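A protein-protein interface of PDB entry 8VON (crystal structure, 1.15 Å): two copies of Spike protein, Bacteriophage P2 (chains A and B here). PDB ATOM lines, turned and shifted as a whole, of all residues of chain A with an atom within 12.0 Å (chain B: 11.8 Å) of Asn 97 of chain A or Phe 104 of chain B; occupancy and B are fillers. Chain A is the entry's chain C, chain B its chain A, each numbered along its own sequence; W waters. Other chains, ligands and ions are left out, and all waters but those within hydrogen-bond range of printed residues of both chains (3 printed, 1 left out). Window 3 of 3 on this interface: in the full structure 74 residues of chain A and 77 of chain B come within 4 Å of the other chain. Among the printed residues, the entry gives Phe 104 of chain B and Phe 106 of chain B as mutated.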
ATOM      1  N   VAL A  77      -5.798  -5.753 -10.069  1.00  0.00           N
ATOM      2  CA  VAL A  77      -5.315  -6.807  -9.191  1.00  0.00           C
ATOM      3  C   VAL A  77      -4.672  -7.867 -10.072  1.00  0.00           C
ATOM      4  O   VAL A  77      -5.312  -8.368 -10.998  1.00  0.00           O
ATOM      5  CB  VAL A  77      -6.453  -7.414  -8.362  1.00  0.00           C
ATOM      6  CG1 VAL A  77      -5.945  -8.562  -7.521  1.00  0.00           C
ATOM      7  CG2 VAL A  77      -7.127  -6.369  -7.503  1.00  0.00           C
ATOM      8  N   GLN A  78      -3.413  -8.193  -9.816  1.00  0.00           N
ATOM      9  CA  GLN A  78      -2.644  -9.028 -10.733  1.00  0.00           C
ATOM     10  C   GLN A  78      -2.663 -10.514 -10.411  1.00  0.00           C
ATOM     11  O   GLN A  78      -2.562 -11.317 -11.345  1.00  0.00           O
ATOM     12  CB  GLN A  78      -1.187  -8.578 -10.744  1.00  0.00           C
ATOM     13  CG  GLN A  78      -1.010  -7.133 -11.146  1.00  0.00           C
ATOM     14  CD  GLN A  78       0.423  -6.679 -10.950  1.00  0.00           C
ATOM     15  OE1 GLN A  78       1.000  -6.873  -9.875  1.00  0.00           O
ATOM     16  NE2 GLN A  78       0.965  -5.968 -11.932  1.00  0.00           N
ATOM     17  N   GLY A  80      -4.716 -12.154  -7.628  1.00  0.00           N
ATOM     18  CA  GLY A  80      -5.812 -12.704  -6.866  1.00  0.00           C
ATOM     19  C   GLY A  80      -6.126 -11.882  -5.633  1.00  0.00           C
ATOM     20  O   GLY A  80      -5.464 -10.902  -5.295  1.00  0.00           O
ATOM     21  N   GLU A  93     -20.773  -3.471 -16.276  1.00  0.00           N
ATOM     22  CA  GLU A  93     -20.897  -4.917 -16.295  1.00  0.00           C
ATOM     23  C   GLU A  93     -19.756  -5.551 -15.520  1.00  0.00           C
ATOM     24  O   GLU A  93     -18.650  -5.007 -15.428  1.00  0.00           O
ATOM     25  CB  GLU A  93     -20.853  -5.461 -17.717  1.00  0.00           C
ATOM     26  CG  GLU A  93     -22.057  -5.086 -18.567  1.00  0.00           C
ATOM     27  CD  GLU A  93     -23.411  -5.617 -18.041  1.00  0.00           C
ATOM     28  OE1 GLU A  93     -24.469  -5.201 -18.566  1.00  0.00           O
ATOM     29  OE2 GLU A  93     -23.424  -6.444 -17.106  1.00  0.00           O
ATOM     30  N   LEU A  94     -20.043  -6.724 -14.976  1.00  0.00           N
ATOM     31  CA  LEU A  94     -19.050  -7.600 -14.383  1.00  0.00           C
ATOM     32  C   LEU A  94     -18.849  -8.739 -15.368  1.00  0.00           C
ATOM     33  O   LEU A  94     -19.816  -9.396 -15.767  1.00  0.00           O
ATOM     34  CB  LEU A  94     -19.562  -8.114 -13.042  1.00  0.00           C
ATOM     35  CG  LEU A  94     -18.685  -9.097 -12.289  1.00  0.00           C
ATOM     36  CD1 LEU A  94     -17.328  -8.472 -12.057  1.00  0.00           C
ATOM     37  CD2 LEU A  94     -19.350  -9.462 -10.970  1.00  0.00           C
ATOM     38  N   SER A  95     -17.614  -8.936 -15.804  1.00  0.00           N
ATOM     39  CA  SER A  95     -17.246 -10.021 -16.698  1.00  0.00           C
ATOM     40  C   SER A  95     -16.289 -10.962 -15.992  1.00  0.00           C
ATOM     41  O   SER A  95     -15.480 -10.526 -15.169  1.00  0.00           O
ATOM     42  CB  SER A  95     -16.577  -9.467 -17.947  1.00  0.00           C
ATOM     43  OG  SER A  95     -17.449  -8.561 -18.585  1.00  0.00           O
ATOM     44  N   SER A  96     -16.373 -12.250 -16.317  1.00  0.00           N
ATOM     45  CA  SER A  96     -15.430 -13.196 -15.748  1.00  0.00           C
ATOM     46  C   SER A  96     -15.077 -14.213 -16.820  1.00  0.00           C
ATOM     47  O   SER A  96     -15.962 -14.790 -17.469  1.00  0.00           O
ATOM     48  CB  SER A  96     -16.001 -13.860 -14.494  1.00  0.00           C
ATOM     49  OG  SER A  96     -15.144 -14.889 -14.053  1.00  0.00           O
ATOM     50  N   ASN A  97     -13.776 -14.378 -17.036  1.00  0.00           N
ATOM     51  CA  ASN A  97     -13.250 -15.374 -17.962  1.00  0.00           C
ATOM     52  C   ASN A  97     -13.831 -15.224 -19.362  1.00  0.00           C
ATOM     53  O   ASN A  97     -14.111 -16.210 -20.044  1.00  0.00           O
ATOM     54  CB  ASN A  97     -13.378 -16.789 -17.395  1.00  0.00           C
ATOM     55  CG  ASN A  97     -12.538 -16.955 -16.135  1.00  0.00           C
ATOM     56  OD1 ASN A  97     -11.360 -16.580 -16.131  1.00  0.00           O
ATOM     57  ND2 ASN A  97     -13.118 -17.502 -15.066  1.00  0.00           N
ATOM     58  N   GLY A  98     -13.966 -13.979 -19.809  1.00  0.00           N
ATOM     59  CA  GLY A  98     -14.294 -13.706 -21.189  1.00  0.00           C
ATOM     60  C   GLY A  98     -15.761 -13.563 -21.482  1.00  0.00           C
ATOM     61  O   GLY A  98     -16.137 -13.448 -22.658  1.00  0.00           O
ATOM     62  N   LYS A  99     -16.605 -13.561 -20.462  1.00  0.00           N
ATOM     63  CA  LYS A  99     -18.031 -13.429 -20.665  1.00  0.00           C
ATOM     64  C   LYS A  99     -18.628 -12.473 -19.651  1.00  0.00           C
ATOM     65  O   LYS A  99     -18.271 -12.479 -18.471  1.00  0.00           O
ATOM     66  CB  LYS A  99     -18.717 -14.787 -20.528  1.00  0.00           C
ATOM     67  CG  LYS A  99     -18.191 -15.826 -21.495  1.00  0.00           C
ATOM     68  CD  LYS A  99     -19.161 -16.982 -21.636  1.00  0.00           C
ATOM     69  CE  LYS A  99     -18.738 -17.934 -22.741  1.00  0.00           C
ATOM     70  NZ  LYS A  99     -19.457 -17.663 -24.018  1.00  0.00           N
ATOM     71  N   VAL A 100     -19.567 -11.663 -20.127  1.00  0.00           N
ATOM     72  CA  VAL A 100     -20.359 -10.840 -19.234  1.00  0.00           C
ATOM     73  C   VAL A 100     -21.208 -11.757 -18.367  1.00  0.00           C
ATOM     74  O   VAL A 100     -21.869 -12.672 -18.874  1.00  0.00           O
ATOM     75  CB  VAL A 100     -21.233  -9.880 -20.047  1.00  0.00           C
ATOM     76  CG1 VAL A 100     -22.210  -9.156 -19.126  1.00  0.00           C
ATOM     77  CG2 VAL A 100     -20.369  -8.936 -20.826  1.00  0.00           C
ATOM     78  N   LEU A 101     -21.210 -11.507 -17.064  1.00  0.00           N
ATOM     79  CA  LEU A 101     -22.025 -12.285 -16.140  1.00  0.00           C
ATOM     80  C   LEU A 101     -23.428 -11.694 -16.074  1.00  0.00           C
ATOM     81  O   LEU A 101     -24.417 -12.445 -16.090  1.00  0.00           O
ATOM     82  CB  LEU A 101     -21.395 -12.288 -14.752  1.00  0.00           C
ATOM     83  CG  LEU A 101     -19.976 -12.858 -14.666  1.00  0.00           C
ATOM     84  CD1 LEU A 101     -19.525 -12.954 -13.217  1.00  0.00           C
ATOM     85  CD2 LEU A 101     -19.895 -14.224 -15.343  1.00  0.00           C
ATOM     86  N   ILE B  87     -16.003  -4.049 -14.555  1.00  0.00           N
ATOM     87  CA  ILE B  87     -14.991  -4.851 -13.879  1.00  0.00           C
ATOM     88  C   ILE B  87     -14.796  -6.117 -14.698  1.00  0.00           C
ATOM     89  O   ILE B  87     -15.761  -6.843 -14.942  1.00  0.00           O
ATOM     90  CB  ILE B  87     -15.411  -5.200 -12.438  1.00  0.00           C
ATOM     91  CG1 ILE B  87     -15.679  -3.939 -11.602  1.00  0.00           C
ATOM     92  CG2 ILE B  87     -14.361  -6.084 -11.786  1.00  0.00           C
ATOM     93  CD1 ILE B  87     -14.460  -3.085 -11.320  1.00  0.00           C
ATOM     94  N   GLU B  88     -13.561  -6.370 -15.129  1.00  0.00           N
ATOM     95  CA  GLU B  88     -13.205  -7.537 -15.922  1.00  0.00           C
ATOM     96  C   GLU B  88     -12.309  -8.462 -15.111  1.00  0.00           C
ATOM     97  O   GLU B  88     -11.193  -8.080 -14.741  1.00  0.00           O
ATOM     98  CB  GLU B  88     -12.477  -7.125 -17.196  1.00  0.00           C
ATOM     99  CG  GLU B  88     -13.319  -6.378 -18.210  1.00  0.00           C
ATOM    100  CD  GLU B  88     -12.471  -5.595 -19.208  1.00  0.00           C
ATOM    101  OE1 GLU B  88     -12.841  -4.451 -19.553  1.00  0.00           O
ATOM    102  OE2 GLU B  88     -11.409  -6.113 -19.613  1.00  0.00           O
ATOM    103  N   HIS B  89     -12.803  -9.662 -14.834  1.00  0.00           N
ATOM    104  CA  HIS B  89     -12.071 -10.684 -14.113  1.00  0.00           C
ATOM    105  C   HIS B  89     -11.617 -11.755 -15.096  1.00  0.00           C
ATOM    106  O   HIS B  89     -12.393 -12.181 -15.951  1.00  0.00           O
ATOM    107  CB  HIS B  89     -12.968 -11.321 -13.059  1.00  0.00           C
ATOM    108  CG  HIS B  89     -12.394 -12.572 -12.503  1.00  0.00           C
ATOM    109  ND1 HIS B  89     -12.942 -13.818 -12.745  1.00  0.00           N
ATOM    110  CD2 HIS B  89     -11.267 -12.774 -11.784  1.00  0.00           C
ATOM    111  CE1 HIS B  89     -12.185 -14.728 -12.159  1.00  0.00           C
ATOM    112  NE2 HIS B  89     -11.163 -14.123 -11.577  1.00  0.00           N
ATOM    113  N   THR B  90     -10.360 -12.188 -14.975  1.00  0.00           N
ATOM    114  CA  THR B  90      -9.831 -13.253 -15.820  1.00  0.00           C
ATOM    115  C   THR B  90      -8.840 -14.094 -15.028  1.00  0.00           C
ATOM    116  O   THR B  90      -8.349 -13.681 -13.980  1.00  0.00           O
ATOM    117  CB  THR B  90      -9.111 -12.694 -17.064  1.00  0.00           C
ATOM    118  OG1 THR B  90      -7.995 -11.888 -16.651  1.00  0.00           O
ATOM    119  CG2 THR B  90     -10.046 -11.879 -17.952  1.00  0.00           C
ATOM    120  N   GLY B  91      -8.525 -15.271 -15.553  1.00  0.00           N
ATOM    121  CA  GLY B  91      -7.368 -16.003 -15.084  1.00  0.00           C
ATOM    122  C   GLY B  91      -7.531 -16.699 -13.764  1.00  0.00           C
ATOM    123  O   GLY B  91      -6.542 -16.914 -13.059  1.00  0.00           O
ATOM    124  N   GLY B  92      -8.752 -17.058 -13.402  1.00  0.00           N
ATOM    125  CA  GLY B  92      -8.959 -17.836 -12.202  1.00  0.00           C
ATOM    126  C   GLY B  92     -10.436 -17.984 -11.914  1.00  0.00           C
ATOM    127  O   GLY B  92     -11.282 -17.703 -12.756  1.00  0.00           O
ATOM    128  N   GLU B  93     -10.715 -18.422 -10.700  1.00  0.00           N
ATOM    129  CA  GLU B  93     -12.068 -18.665 -10.243  1.00  0.00           C
ATOM    130  C   GLU B  93     -12.603 -17.462  -9.492  1.00  0.00           C
ATOM    131  O   GLU B  93     -11.885 -16.834  -8.712  1.00  0.00           O
ATOM    132  CB  GLU B  93     -12.072 -19.856  -9.291  1.00  0.00           C
ATOM    133  CG  GLU B  93     -11.539 -21.122  -9.913  1.00  0.00           C
ATOM    134  CD  GLU B  93     -11.320 -22.201  -8.895  1.00  0.00           C
ATOM    135  OE1 GLU B  93     -10.780 -21.882  -7.808  1.00  0.00           O
ATOM    136  OE2 GLU B  93     -11.700 -23.349  -9.176  1.00  0.00           O
ATOM    137  N   LEU B  94     -13.874 -17.162  -9.721  1.00  0.00           N
ATOM    138  CA  LEU B  94     -14.611 -16.169  -8.957  1.00  0.00           C
ATOM    139  C   LEU B  94     -15.582 -16.932  -8.070  1.00  0.00           C
ATOM    140  O   LEU B  94     -16.315 -17.790  -8.562  1.00  0.00           O
ATOM    141  CB  LEU B  94     -15.343 -15.234  -9.919  1.00  0.00           C
ATOM    142  CG  LEU B  94     -16.212 -14.158  -9.285  1.00  0.00           C
ATOM    143  CD1 LEU B  94     -15.369 -13.185  -8.480  1.00  0.00           C
ATOM    144  CD2 LEU B  94     -16.968 -13.406 -10.387  1.00  0.00           C
ATOM    145  N   SER B  95     -15.558 -16.668  -6.765  1.00  0.00           N
ATOM    146  CA  SER B  95     -16.423 -17.381  -5.848  1.00  0.00           C
ATOM    147  C   SER B  95     -17.051 -16.409  -4.872  1.00  0.00           C
ATOM    148  O   SER B  95     -16.489 -15.347  -4.573  1.00  0.00           O
ATOM    149  CB  SER B  95     -15.685 -18.484  -5.084  1.00  0.00           C
ATOM    150  OG  SER B  95     -14.653 -17.945  -4.301  1.00  0.00           O
ATOM    151  N   SER B  96     -18.210 -16.808  -4.345  1.00  0.00           N
ATOM    152  CA  SER B  96     -18.846 -16.055  -3.280  1.00  0.00           C
ATOM    153  C   SER B  96     -19.360 -17.036  -2.233  1.00  0.00           C
ATOM    154  O   SER B  96     -20.104 -17.976  -2.550  1.00  0.00           O
ATOM    155  CB  SER B  96     -19.950 -15.149  -3.816  1.00  0.00           C
ATOM    156  OG  SER B  96     -20.616 -14.518  -2.743  1.00  0.00           O
ATOM    157  N   GLY B  98     -17.912 -19.415  -0.783  1.00  0.00           N
ATOM    158  CA  GLY B  98     -17.484 -20.766  -1.048  1.00  0.00           C
ATOM    159  C   GLY B  98     -18.053 -21.374  -2.303  1.00  0.00           C
ATOM    160  O   GLY B  98     -17.648 -22.481  -2.667  1.00  0.00           O
ATOM    161  N   LYS B  99     -18.947 -20.680  -2.998  1.00  0.00           N
ATOM    162  CA  LYS B  99     -19.564 -21.196  -4.209  1.00  0.00           C
ATOM    163  C   LYS B  99     -18.826 -20.622  -5.404  1.00  0.00           C
ATOM    164  O   LYS B  99     -18.806 -19.400  -5.603  1.00  0.00           O
ATOM    165  CB  LYS B  99     -21.035 -20.802  -4.259  1.00  0.00           C
ATOM    166  CG  LYS B  99     -21.770 -21.153  -2.966  1.00  0.00           C
ATOM    167  CD  LYS B  99     -23.269 -21.332  -3.149  1.00  0.00           C
ATOM    168  CE  LYS B  99     -23.917 -22.105  -1.987  1.00  0.00           C
ATOM    169  NZ  LYS B  99     -23.130 -23.266  -1.501  1.00  0.00           N
ATOM    170  N   VAL B 100     -18.199 -21.496  -6.178  1.00  0.00           N
ATOM    171  CA  VAL B 100     -17.481 -21.088  -7.372  1.00  0.00           C
ATOM    172  C   VAL B 100     -18.516 -20.779  -8.441  1.00  0.00           C
ATOM    173  O   VAL B 100     -19.338 -21.633  -8.789  1.00  0.00           O
ATOM    174  CB  VAL B 100     -16.500 -22.176  -7.823  1.00  0.00           C
ATOM    175  CG1 VAL B 100     -15.855 -21.783  -9.134  1.00  0.00           C
ATOM    176  CG2 VAL B 100     -15.454 -22.420  -6.753  1.00  0.00           C
ATOM    177  N   LEU B 101     -18.495 -19.552  -8.946  1.00  0.00           N
ATOM    178  CA  LEU B 101     -19.444 -19.164  -9.975  1.00  0.00           C
ATOM    179  C   LEU B 101     -19.077 -19.876 -11.273  1.00  0.00           C
ATOM    180  O   LEU B 101     -17.900 -20.123 -11.566  1.00  0.00           O
ATOM    181  CB  LEU B 101     -19.434 -17.648 -10.152  1.00  0.00           C
ATOM    182  CG  LEU B 101     -19.717 -16.820  -8.894  1.00  0.00           C
ATOM    183  CD1 LEU B 101     -20.026 -15.365  -9.251  1.00  0.00           C
ATOM    184  CD2 LEU B 101     -20.855 -17.387  -8.061  1.00  0.00           C
ATOM    185  N   HIS B 102     -20.101 -20.219 -12.049  1.00  0.00           N
ATOM    186  CA  HIS B 102     -19.917 -21.016 -13.261  1.00  0.00           C
ATOM    187  C   HIS B 102     -19.505 -20.098 -14.413  1.00  0.00           C
ATOM    188  O   HIS B 102     -20.269 -19.811 -15.337  1.00  0.00           O
ATOM    189  CB  HIS B 102     -21.198 -21.776 -13.570  1.00  0.00           C
ATOM    190  CG  HIS B 102     -21.029 -22.923 -14.524  1.00  0.00           C
ATOM    191  ND1 HIS B 102     -19.813 -23.282 -15.065  1.00  0.00           N
ATOM    192  CD2 HIS B 102     -21.933 -23.795 -15.028  1.00  0.00           C
ATOM    193  CE1 HIS B 102     -19.975 -24.321 -15.864  1.00  0.00           C
ATOM    194  NE2 HIS B 102     -21.252 -24.653 -15.856  1.00  0.00           N
ATOM    195  N   THR B 103     -18.253 -19.650 -14.349  1.00  0.00           N
ATOM    196  CA  THR B 103     -17.678 -18.766 -15.356  1.00  0.00           C
ATOM    197  C   THR B 103     -16.669 -19.473 -16.246  1.00  0.00           C
ATOM    198  O   THR B 103     -16.057 -18.830 -17.109  1.00  0.00           O
ATOM    199  CB  THR B 103     -17.048 -17.521 -14.705  1.00  0.00           C
ATOM    200  OG1 THR B 103     -15.799 -17.828 -14.063  1.00  0.00           O
ATOM    201  CG2 THR B 103     -17.979 -16.925 -13.658  1.00  0.00           C
ATOM    202  N   PHE B 104     -16.487 -20.778 -16.066  1.00  0.00           N
ATOM    203  CA  PHE B 104     -15.593 -21.577 -16.888  1.00  0.00           C
ATOM    204  C   PHE B 104     -16.117 -23.007 -16.894  1.00  0.00           C
ATOM    205  O   PHE B 104     -17.085 -23.339 -16.202  1.00  0.00           O
ATOM    206  CB  PHE B 104     -14.155 -21.485 -16.366  1.00  0.00           C
ATOM    207  CG  PHE B 104     -13.989 -21.986 -14.960  1.00  0.00           C
ATOM    208  CD1 PHE B 104     -14.162 -21.129 -13.884  1.00  0.00           C
ATOM    209  CD2 PHE B 104     -13.654 -23.307 -14.713  1.00  0.00           C
ATOM    210  CE1 PHE B 104     -14.010 -21.580 -12.591  1.00  0.00           C
ATOM    211  CE2 PHE B 104     -13.498 -23.767 -13.416  1.00  0.00           C
ATOM    212  CZ  PHE B 104     -13.675 -22.901 -12.353  1.00  0.00           C
ATOM    213  N   LYS B 105     -15.460 -23.861 -17.674  1.00  0.00           N
ATOM    214  CA  LYS B 105     -15.916 -25.233 -17.862  1.00  0.00           C
ATOM    215  C   LYS B 105     -15.776 -26.020 -16.563  1.00  0.00           C
ATOM    216  O   LYS B 105     -14.679 -26.103 -15.998  1.00  0.00           O
ATOM    217  CB  LYS B 105     -15.085 -25.902 -18.952  1.00  0.00           C
ATOM    218  CG  LYS B 105     -15.197 -25.277 -20.336  1.00  0.00           C
ATOM    219  CD  LYS B 105     -14.007 -25.683 -21.210  1.00  0.00           C
ATOM    220  CE  LYS B 105     -13.959 -24.913 -22.524  1.00  0.00           C
ATOM    221  NZ  LYS B 105     -15.100 -25.242 -23.425  1.00  0.00           N
ATOM    222  N   PHE B 106     -16.878 -26.613 -16.107  1.00  0.00           N
ATOM    223  CA  PHE B 106     -16.868 -27.502 -14.949  1.00  0.00           C
ATOM    224  C   PHE B 106     -16.786 -28.949 -15.432  1.00  0.00           C
ATOM    225  O   PHE B 106     -17.435 -29.307 -16.414  1.00  0.00           O
ATOM    226  CB  PHE B 106     -18.138 -27.328 -14.120  1.00  0.00           C
ATOM    227  CG  PHE B 106     -18.175 -26.064 -13.299  1.00  0.00           C
ATOM    228  CD1 PHE B 106     -17.099 -25.181 -13.274  1.00  0.00           C
ATOM    229  CD2 PHE B 106     -19.296 -25.764 -12.540  1.00  0.00           C
ATOM    230  CE1 PHE B 106     -17.145 -24.030 -12.510  1.00  0.00           C
ATOM    231  CE2 PHE B 106     -19.350 -24.612 -11.779  1.00  0.00           C
ATOM    232  CZ  PHE B 106     -18.269 -23.743 -11.759  1.00  0.00           C
HETATM  233  O   HOH W   1      -9.606 -16.022 -18.102  1.00  0.00           O
HETATM  234  O   HOH W   2     -17.802 -16.777 -17.799  1.00  0.00           O
HETATM  235  O   HOH W   3     -17.022  -5.861 -17.799  1.00  0.00           O
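Water W1 bridges the side-chain amide oxygen (OD1) of Asn 97 of chain A and the backbone NH (N) of Gly 91 of chain B. Water W2 lies within hydrogen-bond range of the backbone carbonyl oxygen of Ser 96 of chain A (2.7 Å) and the backbone carbonyl oxygen of Thr 103 of chain B (2.8 Å). Water W3 lies within hydrogen-bond range of OG of Ser 95 of chain A, O of Glu 93 of chain A and O of Ile 87 of chain B.
Of the 19 printed residues of chain B, 9 touch a printed residue of chain A. Hydrophobic or aromatic side chains of chain B within 4 Å of the printed part of chain A: Ile 87, His 89, Leu 94 and Phe 104. Of the 12 printed residues of chain A, 6 touch a printed residue of chain B. Hydrophobic or aromatic side chains of chain A that line the printed part of chain B: Leu 94 and Leu 101.
The backbone carbonyl oxygen (O) of Glu 93 of chain A sits at hydrogen-bond distance from the backbone NH (N) of Ile 87 of chain B. The backbone carbonyl oxygen (O) of Ile 87 of chain B sits at hydrogen-bond distance from the backbone NH (N) of Ser 95 of chain A, 2.9 Å away. The backbone NH (N) of His 89 of chain B sits at hydrogen-bond distance from the backbone carbonyl oxygen (O) of Ser 95 of chain A. The side-chain hydroxyl (OG) of Ser 96 of chain A sits at hydrogen-bond distance from a ring nitrogen (ND1) of His 89 of chain B. The backbone carbonyl oxygen of His 89 of chain B sits at hydrogen-bond distance from the backbone NH of Asn 97 of chain A, at 2.8 Å. OD1 of Asn 97 of chain A lies within hydrogen-bond range of N of Gly 91 of chain B (3.2 Å). The side-chain amide nitrogen of Asn 97 of chain A lies within hydrogen-bond range of the backbone carbonyl oxygen of Gly 92 of chain B, 3.0 Å away. The side-chain hydroxyl of Ser 96 of chain A is in hydrogen-bond range of the side-chain hydroxyl of Thr 103 of chain B. The side-chain hydroxyl (OG1) of Thr 103 of chain B lies within hydrogen-bond range of the side-chain amide nitrogen (ND2) of Asn 97 of chain A (2.9 Å).
Asn 97 of chain A touches six residues of chain B. Of chain B, only His 89 (2.8 Å) and Thr 103 (3.0 Å) come within 4 Å of Ser 96 of chain A. No residue of chain B comes within 4 Å of Gly 98 of chain A. No residue of chain B comes within 4 Å of Lys 99 of chain A. Of chain A, only Asn 97 comes within 4 Å of Thr 90 of chain B. Of chain A, only Asn 97 comes within 4 Å of Gly 91 of chain B. No residue of chain A comes within 4 Å of Glu 93 of chain B. No residue of chain A comes within 4 Å of Val 100 of chain B. No residue of chain A comes within 4 Å of His 102 of chain B. No residue of chain A comes within 4 Å of Lys 105 of chain B. Phe 106 of chain B touches none of the printed residues of chain A. Of the printed residues of chain B, Ser 95 of chain A touches Ile 87 (2.9 Å), Glu 88 (3.8 Å) and His 89 (2.8 Å). Printed residues of chain A within 4 Å of Glu 88 of chain B: Ser 95. Printed residues of chain B within 4 Å of Leu 94 of chain A: Ile 87. Of the printed residues of chain B, Leu 101 of chain A touches Leu 94 (3.8 Å) and Thr 103 (3.7 Å). Of the printed residues of chain A, Leu 94 of chain B touches Leu 101 (3.8 Å). Gln 78 of chain A touches none of the printed residues of chain B. Leu 101 of chain B touches none of the printed residues of chain A. The nearest residue of chain B that does not touch Asn 97 of chain A is Glu 93 of chain B (5.1 Å). The nearest residue of chain A that does not touch Phe 104 of chain B is Ser 96 of chain A (6.2 Å).
O of Ile 87 of chain B touches CA of Leu 94 of chain A, 3.4 Å away. Glu 88 of chain B touches Ser 95 of chain A. CA of Thr 90 of chain B touches OD1 of Asn 97 of chain A, at 3.7 Å. Phe 104 of chain B touches Asn 97 of chain A. Leu 94 of chain B touches Leu 101 of chain A. Leu 101 of chain A touches Thr 103 of chain B (CD2 to CG2, 3.7 Å).
The backbone NH of Leu 101 of chain B is in hydrogen-bond range of the backbone carbonyl oxygen of Leu 94 of chain B, at 2.8 Å. The backbone carbonyl oxygen (O) of Phe 104 of chain B is in hydrogen-bond range of a ring nitrogen (ND1) of His 102 of chain B (3.0 Å). N of Leu 101 of chain A is in hydrogen-bond range of O of Leu 94 of chain A, at 2.8 Å. The side-chain amide nitrogen (ND2) of Asn 97 of chain A sits at hydrogen-bond distance from the side-chain hydroxyl (OG) of Ser 96 of chain A (3.5 Å).
Leu 101 of chain A touches Leu 94 of chain B, but with the chains exchanged Leu 94 of chain A does not touch Leu 101 of chain B (6.2 Å). 8 positions are printed for both chains. Of the 15 pairs that touch across the chains among the printed residues, none has its exchanged pair printed and touching as well.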
